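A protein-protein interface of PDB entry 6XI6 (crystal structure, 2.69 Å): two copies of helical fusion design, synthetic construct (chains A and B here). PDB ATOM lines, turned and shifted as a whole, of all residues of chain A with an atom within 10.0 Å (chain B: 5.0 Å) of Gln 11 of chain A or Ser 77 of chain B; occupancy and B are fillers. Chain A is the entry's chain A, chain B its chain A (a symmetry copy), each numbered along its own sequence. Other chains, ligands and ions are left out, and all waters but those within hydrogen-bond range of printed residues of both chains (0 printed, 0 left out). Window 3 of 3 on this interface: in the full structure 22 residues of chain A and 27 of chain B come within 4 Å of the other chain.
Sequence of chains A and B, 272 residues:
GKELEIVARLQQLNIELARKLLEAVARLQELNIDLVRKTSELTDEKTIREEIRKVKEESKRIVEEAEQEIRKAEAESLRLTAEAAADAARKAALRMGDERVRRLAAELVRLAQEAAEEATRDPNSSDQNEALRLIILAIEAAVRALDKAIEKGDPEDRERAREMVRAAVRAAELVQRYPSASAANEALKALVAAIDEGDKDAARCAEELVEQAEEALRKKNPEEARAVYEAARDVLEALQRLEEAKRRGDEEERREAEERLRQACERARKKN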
ATOM      1  N   GLU A   3      19.332   2.578  -0.937  1.00  0.00           N
ATOM      2  CA  GLU A   3      19.990   1.286  -1.105  1.00  0.00           C
ATOM      3  C   GLU A   3      18.973   0.156  -1.201  1.00  0.00           C
ATOM      4  O   GLU A   3      19.125  -0.757  -2.023  1.00  0.00           O
ATOM      5  CB  GLU A   3      20.964   1.032   0.047  1.00  0.00           C
ATOM      6  CG  GLU A   3      22.252   1.843  -0.018  1.00  0.00           C
ATOM      7  CD  GLU A   3      22.066   3.285   0.412  1.00  0.00           C
ATOM      8  OE1 GLU A   3      21.051   3.585   1.075  1.00  0.00           O
ATOM      9  OE2 GLU A   3      22.937   4.119   0.088  1.00  0.00           O
ATOM     10  N   LEU A   4      17.926   0.198  -0.373  1.00  0.00           N
ATOM     11  CA  LEU A   4      16.902  -0.840  -0.424  1.00  0.00           C
ATOM     12  C   LEU A   4      16.080  -0.762  -1.704  1.00  0.00           C
ATOM     13  O   LEU A   4      15.584  -1.789  -2.181  1.00  0.00           O
ATOM     14  CB  LEU A   4      15.990  -0.743   0.798  1.00  0.00           C
ATOM     15  CG  LEU A   4      16.581  -1.224   2.124  1.00  0.00           C
ATOM     16  CD1 LEU A   4      15.608  -0.980   3.266  1.00  0.00           C
ATOM     17  CD2 LEU A   4      16.955  -2.697   2.038  1.00  0.00           C
ATOM     18  N   GLU A   5      15.924   0.436  -2.271  1.00  0.00           N
ATOM     19  CA  GLU A   5      15.174   0.570  -3.516  1.00  0.00           C
ATOM     20  C   GLU A   5      15.889  -0.123  -4.670  1.00  0.00           C
ATOM     21  O   GLU A   5      15.250  -0.789  -5.492  1.00  0.00           O
ATOM     22  CB  GLU A   5      14.947   2.046  -3.840  1.00  0.00           C
ATOM     23  CG  GLU A   5      14.111   2.794  -2.817  1.00  0.00           C
ATOM     24  CD  GLU A   5      13.891   4.245  -3.201  1.00  0.00           C
ATOM     25  OE1 GLU A   5      14.314   4.636  -4.309  1.00  0.00           O
ATOM     26  OE2 GLU A   5      13.295   4.993  -2.396  1.00  0.00           O
ATOM     27  N   ILE A   6      17.213   0.021  -4.744  1.00  0.00           N
ATOM     28  CA  ILE A   6      17.965  -0.581  -5.841  1.00  0.00           C
ATOM     29  C   ILE A   6      17.941  -2.101  -5.737  1.00  0.00           C
ATOM     30  O   ILE A   6      17.799  -2.803  -6.745  1.00  0.00           O
ATOM     31  CB  ILE A   6      19.404  -0.036  -5.864  1.00  0.00           C
ATOM     32  CG1 ILE A   6      19.393   1.494  -5.850  1.00  0.00           C
ATOM     33  CG2 ILE A   6      20.155  -0.559  -7.081  1.00  0.00           C
ATOM     34  CD1 ILE A   6      18.607   2.115  -6.986  1.00  0.00           C
ATOM     35  N   VAL A   7      18.078  -2.632  -4.520  1.00  0.00           N
ATOM     36  CA  VAL A   7      18.051  -4.080  -4.330  1.00  0.00           C
ATOM     37  C   VAL A   7      16.695  -4.645  -4.736  1.00  0.00           C
ATOM     38  O   VAL A   7      16.605  -5.744  -5.295  1.00  0.00           O
ATOM     39  CB  VAL A   7      18.403  -4.432  -2.872  1.00  0.00           C
ATOM     40  CG1 VAL A   7      18.369  -5.934  -2.660  1.00  0.00           C
ATOM     41  CG2 VAL A   7      19.770  -3.876  -2.510  1.00  0.00           C
ATOM     42  N   ALA A   8      15.622  -3.897  -4.474  1.00  0.00           N
ATOM     43  CA  ALA A   8      14.294  -4.346  -4.881  1.00  0.00           C
ATOM     44  C   ALA A   8      14.162  -4.378  -6.397  1.00  0.00           C
ATOM     45  O   ALA A   8      13.580  -5.314  -6.956  1.00  0.00           O
ATOM     46  CB  ALA A   8      13.224  -3.443  -4.268  1.00  0.00           C
ATOM     47  N   ARG A   9      14.700  -3.365  -7.082  1.00  0.00           N
ATOM     48  CA  ARG A   9      14.606  -3.324  -8.537  1.00  0.00           C
ATOM     49  C   ARG A   9      15.538  -4.340  -9.185  1.00  0.00           C
ATOM     50  O   ARG A   9      15.172  -4.982 -10.177  1.00  0.00           O
ATOM     51  CB  ARG A   9      14.907  -1.913  -9.040  1.00  0.00           C
ATOM     52  CG  ARG A   9      13.746  -0.950  -8.879  1.00  0.00           C
ATOM     53  CD  ARG A   9      14.200   0.392  -8.335  1.00  0.00           C
ATOM     54  NE  ARG A   9      13.072   1.293  -8.121  1.00  0.00           N
ATOM     55  CZ  ARG A   9      12.267   1.246  -7.064  1.00  0.00           C
ATOM     56  NH1 ARG A   9      11.264   2.108  -6.954  1.00  0.00           N
ATOM     57  NH2 ARG A   9      12.459   0.337  -6.118  1.00  0.00           N
ATOM     58  N   LEU A  10      16.748  -4.500  -8.643  1.00  0.00           N
ATOM     59  CA  LEU A  10      17.675  -5.487  -9.191  1.00  0.00           C
ATOM     60  C   LEU A  10      17.157  -6.907  -9.006  1.00  0.00           C
ATOM     61  O   LEU A  10      17.419  -7.774  -9.847  1.00  0.00           O
ATOM     62  CB  LEU A  10      19.051  -5.334  -8.545  1.00  0.00           C
ATOM     63  CG  LEU A  10      19.837  -4.075  -8.920  1.00  0.00           C
ATOM     64  CD1 LEU A  10      21.167  -4.034  -8.190  1.00  0.00           C
ATOM     65  CD2 LEU A  10      20.047  -4.010 -10.423  1.00  0.00           C
ATOM     66  N   GLN A  11      16.425  -7.164  -7.920  1.00  0.00           N
ATOM     67  CA  GLN A  11      15.858  -8.492  -7.716  1.00  0.00           C
ATOM     68  C   GLN A  11      14.713  -8.766  -8.683  1.00  0.00           C
ATOM     69  O   GLN A  11      14.521  -9.913  -9.104  1.00  0.00           O
ATOM     70  CB  GLN A  11      15.388  -8.647  -6.267  1.00  0.00           C
ATOM     71  CG  GLN A  11      14.847 -10.029  -5.925  1.00  0.00           C
ATOM     72  CD  GLN A  11      15.896 -11.123  -6.040  1.00  0.00           C
ATOM     73  OE1 GLN A  11      17.097 -10.853  -6.072  1.00  0.00           O
ATOM     74  NE2 GLN A  11      15.441 -12.369  -6.100  1.00  0.00           N
ATOM     75  N   GLN A  12      13.948  -7.734  -9.046  1.00  0.00           N
ATOM     76  CA  GLN A  12      12.909  -7.908 -10.056  1.00  0.00           C
ATOM     77  C   GLN A  12      13.513  -8.281 -11.404  1.00  0.00           C
ATOM     78  O   GLN A  12      12.933  -9.070 -12.157  1.00  0.00           O
ATOM     79  CB  GLN A  12      12.072  -6.635 -10.178  1.00  0.00           C
ATOM     80  CG  GLN A  12      11.254  -6.300  -8.943  1.00  0.00           C
ATOM     81  CD  GLN A  12      10.483  -5.003  -9.093  1.00  0.00           C
ATOM     82  OE1 GLN A  12      10.528  -4.358 -10.140  1.00  0.00           O
ATOM     83  NE2 GLN A  12       9.770  -4.614  -8.042  1.00  0.00           N
ATOM     84  N   LEU A  13      14.683  -7.721 -11.725  1.00  0.00           N
ATOM     85  CA  LEU A  13      15.354  -8.074 -12.971  1.00  0.00           C
ATOM     86  C   LEU A  13      15.796  -9.532 -12.967  1.00  0.00           C
ATOM     87  O   LEU A  13      15.675 -10.225 -13.984  1.00  0.00           O
ATOM     88  CB  LEU A  13      16.555  -7.157 -13.205  1.00  0.00           C
ATOM     89  CG  LEU A  13      16.271  -5.678 -13.469  1.00  0.00           C
ATOM     90  CD1 LEU A  13      17.570  -4.934 -13.732  1.00  0.00           C
ATOM     91  CD2 LEU A  13      15.308  -5.516 -14.634  1.00  0.00           C
ATOM     92  N   ASN A  14      16.311 -10.014 -11.832  1.00  0.00           N
ATOM     93  CA  ASN A  14      16.768 -11.398 -11.756  1.00  0.00           C
ATOM     94  C   ASN A  14      15.606 -12.373 -11.891  1.00  0.00           C
ATOM     95  O   ASN A  14      15.720 -13.391 -12.583  1.00  0.00           O
ATOM     96  CB  ASN A  14      17.517 -11.632 -10.445  1.00  0.00           C
ATOM     97  CG  ASN A  14      18.725 -10.729 -10.295  1.00  0.00           C
ATOM     98  OD1 ASN A  14      19.317 -10.296 -11.283  1.00  0.00           O
ATOM     99  ND2 ASN A  14      19.098 -10.440  -9.054  1.00  0.00           N
ATOM    100  N   ILE A  15      14.480 -12.081 -11.234  1.00  0.00           N
ATOM    101  CA  ILE A  15      13.304 -12.936 -11.361  1.00  0.00           C
ATOM    102  C   ILE A  15      12.776 -12.901 -12.789  1.00  0.00           C
ATOM    103  O   ILE A  15      12.409 -13.938 -13.358  1.00  0.00           O
ATOM    104  CB  ILE A  15      12.223 -12.513 -10.347  1.00  0.00           C
ATOM    105  CG1 ILE A  15      12.740 -12.675  -8.916  1.00  0.00           C
ATOM    106  CG2 ILE A  15      10.949 -13.320 -10.554  1.00  0.00           C
ATOM    107  CD1 ILE A  15      13.103 -14.099  -8.556  1.00  0.00           C
ATOM    108  N   GLU A  16      12.737 -11.711 -13.393  1.00  0.00           N
ATOM    109  CA  GLU A  16      12.244 -11.591 -14.760  1.00  0.00           C
ATOM    110  C   GLU A  16      13.195 -12.249 -15.752  1.00  0.00           C
ATOM    111  O   GLU A  16      12.753 -12.889 -16.713  1.00  0.00           O
ATOM    112  CB  GLU A  16      12.031 -10.118 -15.111  1.00  0.00           C
ATOM    113  CG  GLU A  16      11.473  -9.882 -16.505  1.00  0.00           C
ATOM    114  CD  GLU A  16      10.076 -10.448 -16.683  1.00  0.00           C
ATOM    115  OE1 GLU A  16       9.351 -10.583 -15.675  1.00  0.00           O
ATOM    116  OE2 GLU A  16       9.705 -10.760 -17.834  1.00  0.00           O
ATOM    117  N   LEU A  17      14.505 -12.106 -15.536  1.00  0.00           N
ATOM    118  CA  LEU A  17      15.468 -12.730 -16.437  1.00  0.00           C
ATOM    119  C   LEU A  17      15.407 -14.250 -16.338  1.00  0.00           C
ATOM    120  O   LEU A  17      15.485 -14.946 -17.357  1.00  0.00           O
ATOM    121  CB  LEU A  17      16.879 -12.227 -16.133  1.00  0.00           C
ATOM    122  CG  LEU A  17      17.964 -12.635 -17.130  1.00  0.00           C
ATOM    123  CD1 LEU A  17      17.593 -12.177 -18.533  1.00  0.00           C
ATOM    124  CD2 LEU A  17      19.314 -12.067 -16.715  1.00  0.00           C
ATOM    125  N   ALA A  18      15.266 -14.781 -15.122  1.00  0.00           N
ATOM    126  CA  ALA A  18      15.096 -16.220 -14.966  1.00  0.00           C
ATOM    127  C   ALA A  18      13.772 -16.690 -15.551  1.00  0.00           C
ATOM    128  O   ALA A  18      13.671 -17.830 -16.020  1.00  0.00           O
ATOM    129  CB  ALA A  18      15.195 -16.607 -13.491  1.00  0.00           C
ATOM    130  N   ARG A  19      12.750 -15.831 -15.534  1.00  0.00           N
ATOM    131  CA  ARG A  19      11.471 -16.189 -16.137  1.00  0.00           C
ATOM    132  C   ARG A  19      11.591 -16.306 -17.652  1.00  0.00           C
ATOM    133  O   ARG A  19      10.993 -17.202 -18.260  1.00  0.00           O
ATOM    134  CB  ARG A  19      10.409 -15.156 -15.761  1.00  0.00           C
ATOM    135  CG  ARG A  19       8.994 -15.526 -16.180  1.00  0.00           C
ATOM    136  CD  ARG A  19       8.194 -16.072 -15.007  1.00  0.00           C
ATOM    137  NE  ARG A  19       8.031 -15.075 -13.951  1.00  0.00           N
ATOM    138  CZ  ARG A  19       7.335 -15.273 -12.837  1.00  0.00           C
ATOM    139  NH1 ARG A  19       6.732 -16.436 -12.626  1.00  0.00           N
ATOM    140  NH2 ARG A  19       7.241 -14.309 -11.931  1.00  0.00           N
ATOM    141  N   ALA A  73      18.970  -6.665 -19.632  1.00  0.00           N
ATOM    142  CA  ALA A  73      18.949  -6.756 -18.176  1.00  0.00           C
ATOM    143  C   ALA A  73      20.260  -6.280 -17.566  1.00  0.00           C
ATOM    144  O   ALA A  73      20.265  -5.746 -16.451  1.00  0.00           O
ATOM    145  CB  ALA A  73      18.649  -8.190 -17.741  1.00  0.00           C
ATOM    146  N   GLU A  76      20.243  -2.343 -17.678  1.00  0.00           N
ATOM    147  CA  GLU A  76      19.346  -1.827 -16.650  1.00  0.00           C
ATOM    148  C   GLU A  76      19.953  -1.973 -15.260  1.00  0.00           C
ATOM    149  O   GLU A  76      19.740  -1.115 -14.397  1.00  0.00           O
ATOM    150  CB  GLU A  76      17.998  -2.545 -16.731  1.00  0.00           C
ATOM    151  CG  GLU A  76      16.932  -2.012 -15.784  1.00  0.00           C
ATOM    152  CD  GLU A  76      16.700  -0.525 -15.942  1.00  0.00           C
ATOM    153  OE1 GLU A  76      17.245   0.249 -15.129  1.00  0.00           O
ATOM    154  OE2 GLU A  76      15.979  -0.130 -16.883  1.00  0.00           O
ATOM    155  N   SER A  77      20.716  -3.045 -15.030  1.00  0.00           N
ATOM    156  CA  SER A  77      21.393  -3.207 -13.748  1.00  0.00           C
ATOM    157  C   SER A  77      22.525  -2.201 -13.592  1.00  0.00           C
ATOM    158  O   SER A  77      22.697  -1.611 -12.518  1.00  0.00           O
ATOM    159  CB  SER A  77      21.920  -4.634 -13.607  1.00  0.00           C
ATOM    160  OG  SER A  77      20.861  -5.575 -13.613  1.00  0.00           O
ATOM    161  N   LEU A  80      21.108   1.240 -12.719  1.00  0.00           N
ATOM    162  CA  LEU A  80      20.704   1.399 -11.326  1.00  0.00           C
ATOM    163  C   LEU A  80      21.913   1.536 -10.409  1.00  0.00           C
ATOM    164  O   LEU A  80      21.888   2.321  -9.454  1.00  0.00           O
ATOM    165  CB  LEU A  80      19.834   0.218 -10.896  1.00  0.00           C
ATOM    166  CG  LEU A  80      18.466   0.112 -11.571  1.00  0.00           C
ATOM    167  CD1 LEU A  80      17.784  -1.194 -11.205  1.00  0.00           C
ATOM    168  CD2 LEU A  80      17.595   1.299 -11.191  1.00  0.00           C
ATOM    169  N   LEU B  10      18.542 -12.763  -0.438  1.00  0.00           N
ATOM    170  CA  LEU B  10      18.120 -12.660  -1.831  1.00  0.00           C
ATOM    171  C   LEU B  10      19.127 -13.308  -2.772  1.00  0.00           C
ATOM    172  O   LEU B  10      18.739 -13.850  -3.813  1.00  0.00           O
ATOM    173  CB  LEU B  10      17.904 -11.196  -2.211  1.00  0.00           C
ATOM    174  CG  LEU B  10      16.697 -10.505  -1.573  1.00  0.00           C
ATOM    175  CD1 LEU B  10      16.616  -9.053  -2.010  1.00  0.00           C
ATOM    176  CD2 LEU B  10      15.417 -11.243  -1.925  1.00  0.00           C
ATOM    177  N   LEU B  13      18.557 -17.029  -2.876  1.00  0.00           N
ATOM    178  CA  LEU B  13      17.441 -17.375  -3.750  1.00  0.00           C
ATOM    179  C   LEU B  13      17.878 -17.424  -5.209  1.00  0.00           C
ATOM    180  O   LEU B  13      17.458 -18.313  -5.958  1.00  0.00           O
ATOM    181  CB  LEU B  13      16.298 -16.377  -3.571  1.00  0.00           C
ATOM    182  CG  LEU B  13      15.580 -16.362  -2.221  1.00  0.00           C
ATOM    183  CD1 LEU B  13      14.444 -15.353  -2.243  1.00  0.00           C
ATOM    184  CD2 LEU B  13      15.065 -17.749  -1.871  1.00  0.00           C
ATOM    185  N   ASN B  14      18.718 -16.475  -5.630  1.00  0.00           N
ATOM    186  CA  ASN B  14      19.169 -16.449  -7.017  1.00  0.00           C
ATOM    187  C   ASN B  14      20.038 -17.658  -7.340  1.00  0.00           C
ATOM    188  O   ASN B  14      19.899 -18.260  -8.412  1.00  0.00           O
ATOM    189  CB  ASN B  14      19.927 -15.152  -7.299  1.00  0.00           C
ATOM    190  CG  ASN B  14      19.080 -13.918  -7.057  1.00  0.00           C
ATOM    191  OD1 ASN B  14      17.856 -13.961  -7.165  1.00  0.00           O
ATOM    192  ND2 ASN B  14      19.731 -12.809  -6.727  1.00  0.00           N
ATOM    193  N   ALA B  73      10.020 -18.341  -5.602  1.00  0.00           N
ATOM    194  CA  ALA B  73      11.187 -17.497  -5.369  1.00  0.00           C
ATOM    195  C   ALA B  73      10.833 -16.018  -5.447  1.00  0.00           C
ATOM    196  O   ALA B  73      11.452 -15.197  -4.761  1.00  0.00           O
ATOM    197  CB  ALA B  73      12.290 -17.833  -6.372  1.00  0.00           C
ATOM    198  N   GLU B  74       9.844 -15.660  -6.271  1.00  0.00           N
ATOM    199  CA  GLU B  74       9.439 -14.262  -6.372  1.00  0.00           C
ATOM    200  C   GLU B  74       8.712 -13.805  -5.115  1.00  0.00           C
ATOM    201  O   GLU B  74       8.947 -12.694  -4.623  1.00  0.00           O
ATOM    202  CB  GLU B  74       8.557 -14.058  -7.604  1.00  0.00           C
ATOM    203  CG  GLU B  74       8.142 -12.614  -7.835  1.00  0.00           C
ATOM    204  CD  GLU B  74       7.188 -12.460  -9.002  1.00  0.00           C
ATOM    205  OE1 GLU B  74       6.550 -13.462  -9.388  1.00  0.00           O
ATOM    206  OE2 GLU B  74       7.078 -11.336  -9.536  1.00  0.00           O
ATOM    207  N   ALA B  75       7.824 -14.647  -4.579  1.00  0.00           N
ATOM    208  CA  ALA B  75       7.102 -14.287  -3.363  1.00  0.00           C
ATOM    209  C   ALA B  75       8.048 -14.165  -2.175  1.00  0.00           C
ATOM    210  O   ALA B  75       7.897 -13.261  -1.345  1.00  0.00           O
ATOM    211  CB  ALA B  75       6.010 -15.316  -3.076  1.00  0.00           C
ATOM    212  N   GLU B  76       9.028 -15.066  -2.079  1.00  0.00           N
ATOM    213  CA  GLU B  76      10.011 -14.979  -1.005  1.00  0.00           C
ATOM    214  C   GLU B  76      10.857 -13.718  -1.127  1.00  0.00           C
ATOM    215  O   GLU B  76      11.243 -13.128  -0.112  1.00  0.00           O
ATOM    216  CB  GLU B  76      10.895 -16.228  -1.007  1.00  0.00           C
ATOM    217  CG  GLU B  76      11.887 -16.311   0.143  1.00  0.00           C
ATOM    218  CD  GLU B  76      11.222 -16.192   1.499  1.00  0.00           C
ATOM    219  OE1 GLU B  76      11.251 -15.087   2.077  1.00  0.00           O
ATOM    220  OE2 GLU B  76      10.665 -17.200   1.981  1.00  0.00           O
ATOM    221  N   SER B  77      11.147 -13.287  -2.358  1.00  0.00           N
ATOM    222  CA  SER B  77      11.884 -12.043  -2.549  1.00  0.00           C
ATOM    223  C   SER B  77      11.032 -10.835  -2.181  1.00  0.00           C
ATOM    224  O   SER B  77      11.516  -9.900  -1.533  1.00  0.00           O
ATOM    225  CB  SER B  77      12.371 -11.936  -3.993  1.00  0.00           C
ATOM    226  OG  SER B  77      13.275 -12.980  -4.308  1.00  0.00           O
ATOM    227  N   LEU B  78       9.759 -10.837  -2.586  1.00  0.00           N
ATOM    228  CA  LEU B  78       8.872  -9.731  -2.241  1.00  0.00           C
ATOM    229  C   LEU B  78       8.601  -9.674  -0.743  1.00  0.00           C
ATOM    230  O   LEU B  78       8.358  -8.589  -0.202  1.00  0.00           O
ATOM    231  CB  LEU B  78       7.558  -9.849  -3.013  1.00  0.00           C
ATOM    232  CG  LEU B  78       7.625  -9.658  -4.529  1.00  0.00           C
ATOM    233  CD1 LEU B  78       6.244  -9.812  -5.144  1.00  0.00           C
ATOM    234  CD2 LEU B  78       8.221  -8.302  -4.874  1.00  0.00           C
ATOM    235  N   ARG B  79       8.636 -10.819  -0.060  1.00  0.00           N
ATOM    236  CA  ARG B  79       8.449 -10.817   1.386  1.00  0.00           C
ATOM    237  C   ARG B  79       9.640 -10.182   2.092  1.00  0.00           C
ATOM    238  O   ARG B  79       9.468  -9.429   3.057  1.00  0.00           O
ATOM    239  CB  ARG B  79       8.218 -12.243   1.887  1.00  0.00           C
ATOM    240  CG  ARG B  79       7.746 -12.332   3.332  1.00  0.00           C
ATOM    241  CD  ARG B  79       8.865 -12.746   4.274  1.00  0.00           C
ATOM    242  NE  ARG B  79       9.222 -14.153   4.119  1.00  0.00           N
ATOM    243  CZ  ARG B  79      10.127 -14.780   4.865  1.00  0.00           C
ATOM    244  NH1 ARG B  79      10.772 -14.124   5.820  1.00  0.00           N
ATOM    245  NH2 ARG B  79      10.390 -16.062   4.653  1.00  0.00           N
ATOM    246  N   LEU B  80      10.856 -10.465   1.618  1.00  0.00           N
ATOM    247  CA  LEU B  80      12.044  -9.881   2.231  1.00  0.00           C
ATOM    248  C   LEU B  80      12.122  -8.382   1.973  1.00  0.00           C
ATOM    249  O   LEU B  80      12.523  -7.614   2.855  1.00  0.00           O
ATOM    250  CB  LEU B  80      13.299 -10.581   1.712  1.00  0.00           C
ATOM    251  CG  LEU B  80      13.469 -12.045   2.121  1.00  0.00           C
ATOM    252  CD1 LEU B  80      14.642 -12.676   1.392  1.00  0.00           C
ATOM    253  CD2 LEU B  80      13.647 -12.155   3.626  1.00  0.00           C
ATOM    254  N   THR B  81      11.743  -7.945   0.769  1.00  0.00           N
ATOM    255  CA  THR B  81      11.779  -6.521   0.456  1.00  0.00           C
ATOM    256  C   THR B  81      10.725  -5.755   1.246  1.00  0.00           C
ATOM    257  O   THR B  81      10.979  -4.638   1.711  1.00  0.00           O
ATOM    258  CB  THR B  81      11.588  -6.311  -1.046  1.00  0.00           C
ATOM    259  OG1 THR B  81      12.694  -6.886  -1.752  1.00  0.00           O
ATOM    260  CG2 THR B  81      11.496  -4.832  -1.377  1.00  0.00           C
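Printed residues of chain B that touch a printed residue of chain A: Leu 10, Asn 14, Glu 74, Ser 77 and Thr 81.
Along chain B the printed residues that touch a printed residue of chain A span positions 10 to 81.
Printed residues of chain A that touch a printed residue of chain B: Val 7, Ala 8, Gln 11, Asn 14, Ile 15 and Arg 19.
Along chain A the printed residues that touch a printed residue of chain B span positions 7 to 19.
Among the printed residues, 8 pairs touch across the chains.
Among the printed residues, Asp or Glu carboxylates within 4 Å of a Lys or Arg side-chain nitrogen of the other chain: Arg 19 of chain A with Glu 74 of chain B (2.8 Å).
Among the printed residues, merely in contact across the chains: Val 7 of chain A with Leu 10 of chain B, Ala 8 of chain A with Thr 81 of chain B, Ile 15 of chain A with Glu 74 of chain B and Gln 11 of chain A with Leu 10 of chain B.
O of Ala 73 of chain B sits at hydrogen-bond distance from OG of Ser 77 of chain B, at 2.9 Å.
The backbone carbonyl oxygen of Leu 10 of chain A sits at hydrogen-bond distance from the side-chain amide nitrogen of Asn 14 of chain A, at 3.2 Å.
The side-chain hydroxyl (OG1) of Thr 81 of chain B sits at hydrogen-bond distance from the backbone carbonyl oxygen (O) of Ser 77 of chain B, at 3.2 Å.
ND2 of Asn 14 of chain B sits at hydrogen-bond distance from O of Leu 10 of chain B, 3.2 Å away.
Printed residues of chain B within 4 Å of Ala 8 of chain A: Thr 81 (3.6 Å).
Of chain B, only Leu 10, Asn 14 and Ser 77 come within 4 Å of Gln 11 of chain A.
Of the printed residues of chain B, Asn 14 of chain A touches Asn 14.
Of the printed residues of chain A, Leu 10 of chain B touches Val 7 and Gln 11.
No residue of chain A comes within 4 Å of Ala 75 of chain B.
Of chain A, only Gln 11 (2.9 Å) comes within 4 Å of Ser 77 of chain B.
No residue of chain A comes within 4 Å of Leu 78 of chain B.
Printed residues of chain A within 4 Å of Thr 81 of chain B: Ala 8 (3.6 Å).
The nearest residue of chain A that does not touch Ser 77 of chain B is Ile 15 of chain A (4.4 Å).
The nearest printed residue of chain A that does not touch Leu 10 of chain B is Ala 8 of chain A (5.8 Å).
NH2 of Arg 19 of chain A lies within salt-bridge range of OE1 of Glu 74 of chain B (2.8 Å).
OG of Ser 77 of chain B sits at hydrogen-bond distance from NE2 of Gln 11 of chain A (2.9 Å).
The side-chain amide oxygen (OD1) of Asn 14 of chain B is in hydrogen-bond range of the side-chain amide nitrogen (NE2) of Gln 11 of chain A (3.1 Å).
ND2 of Asn 14 of chain A lies close to ND2 of Asn 14 of chain B.
Asn 14 of chain A touches its own counterpart, Asn 14 of chain B.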
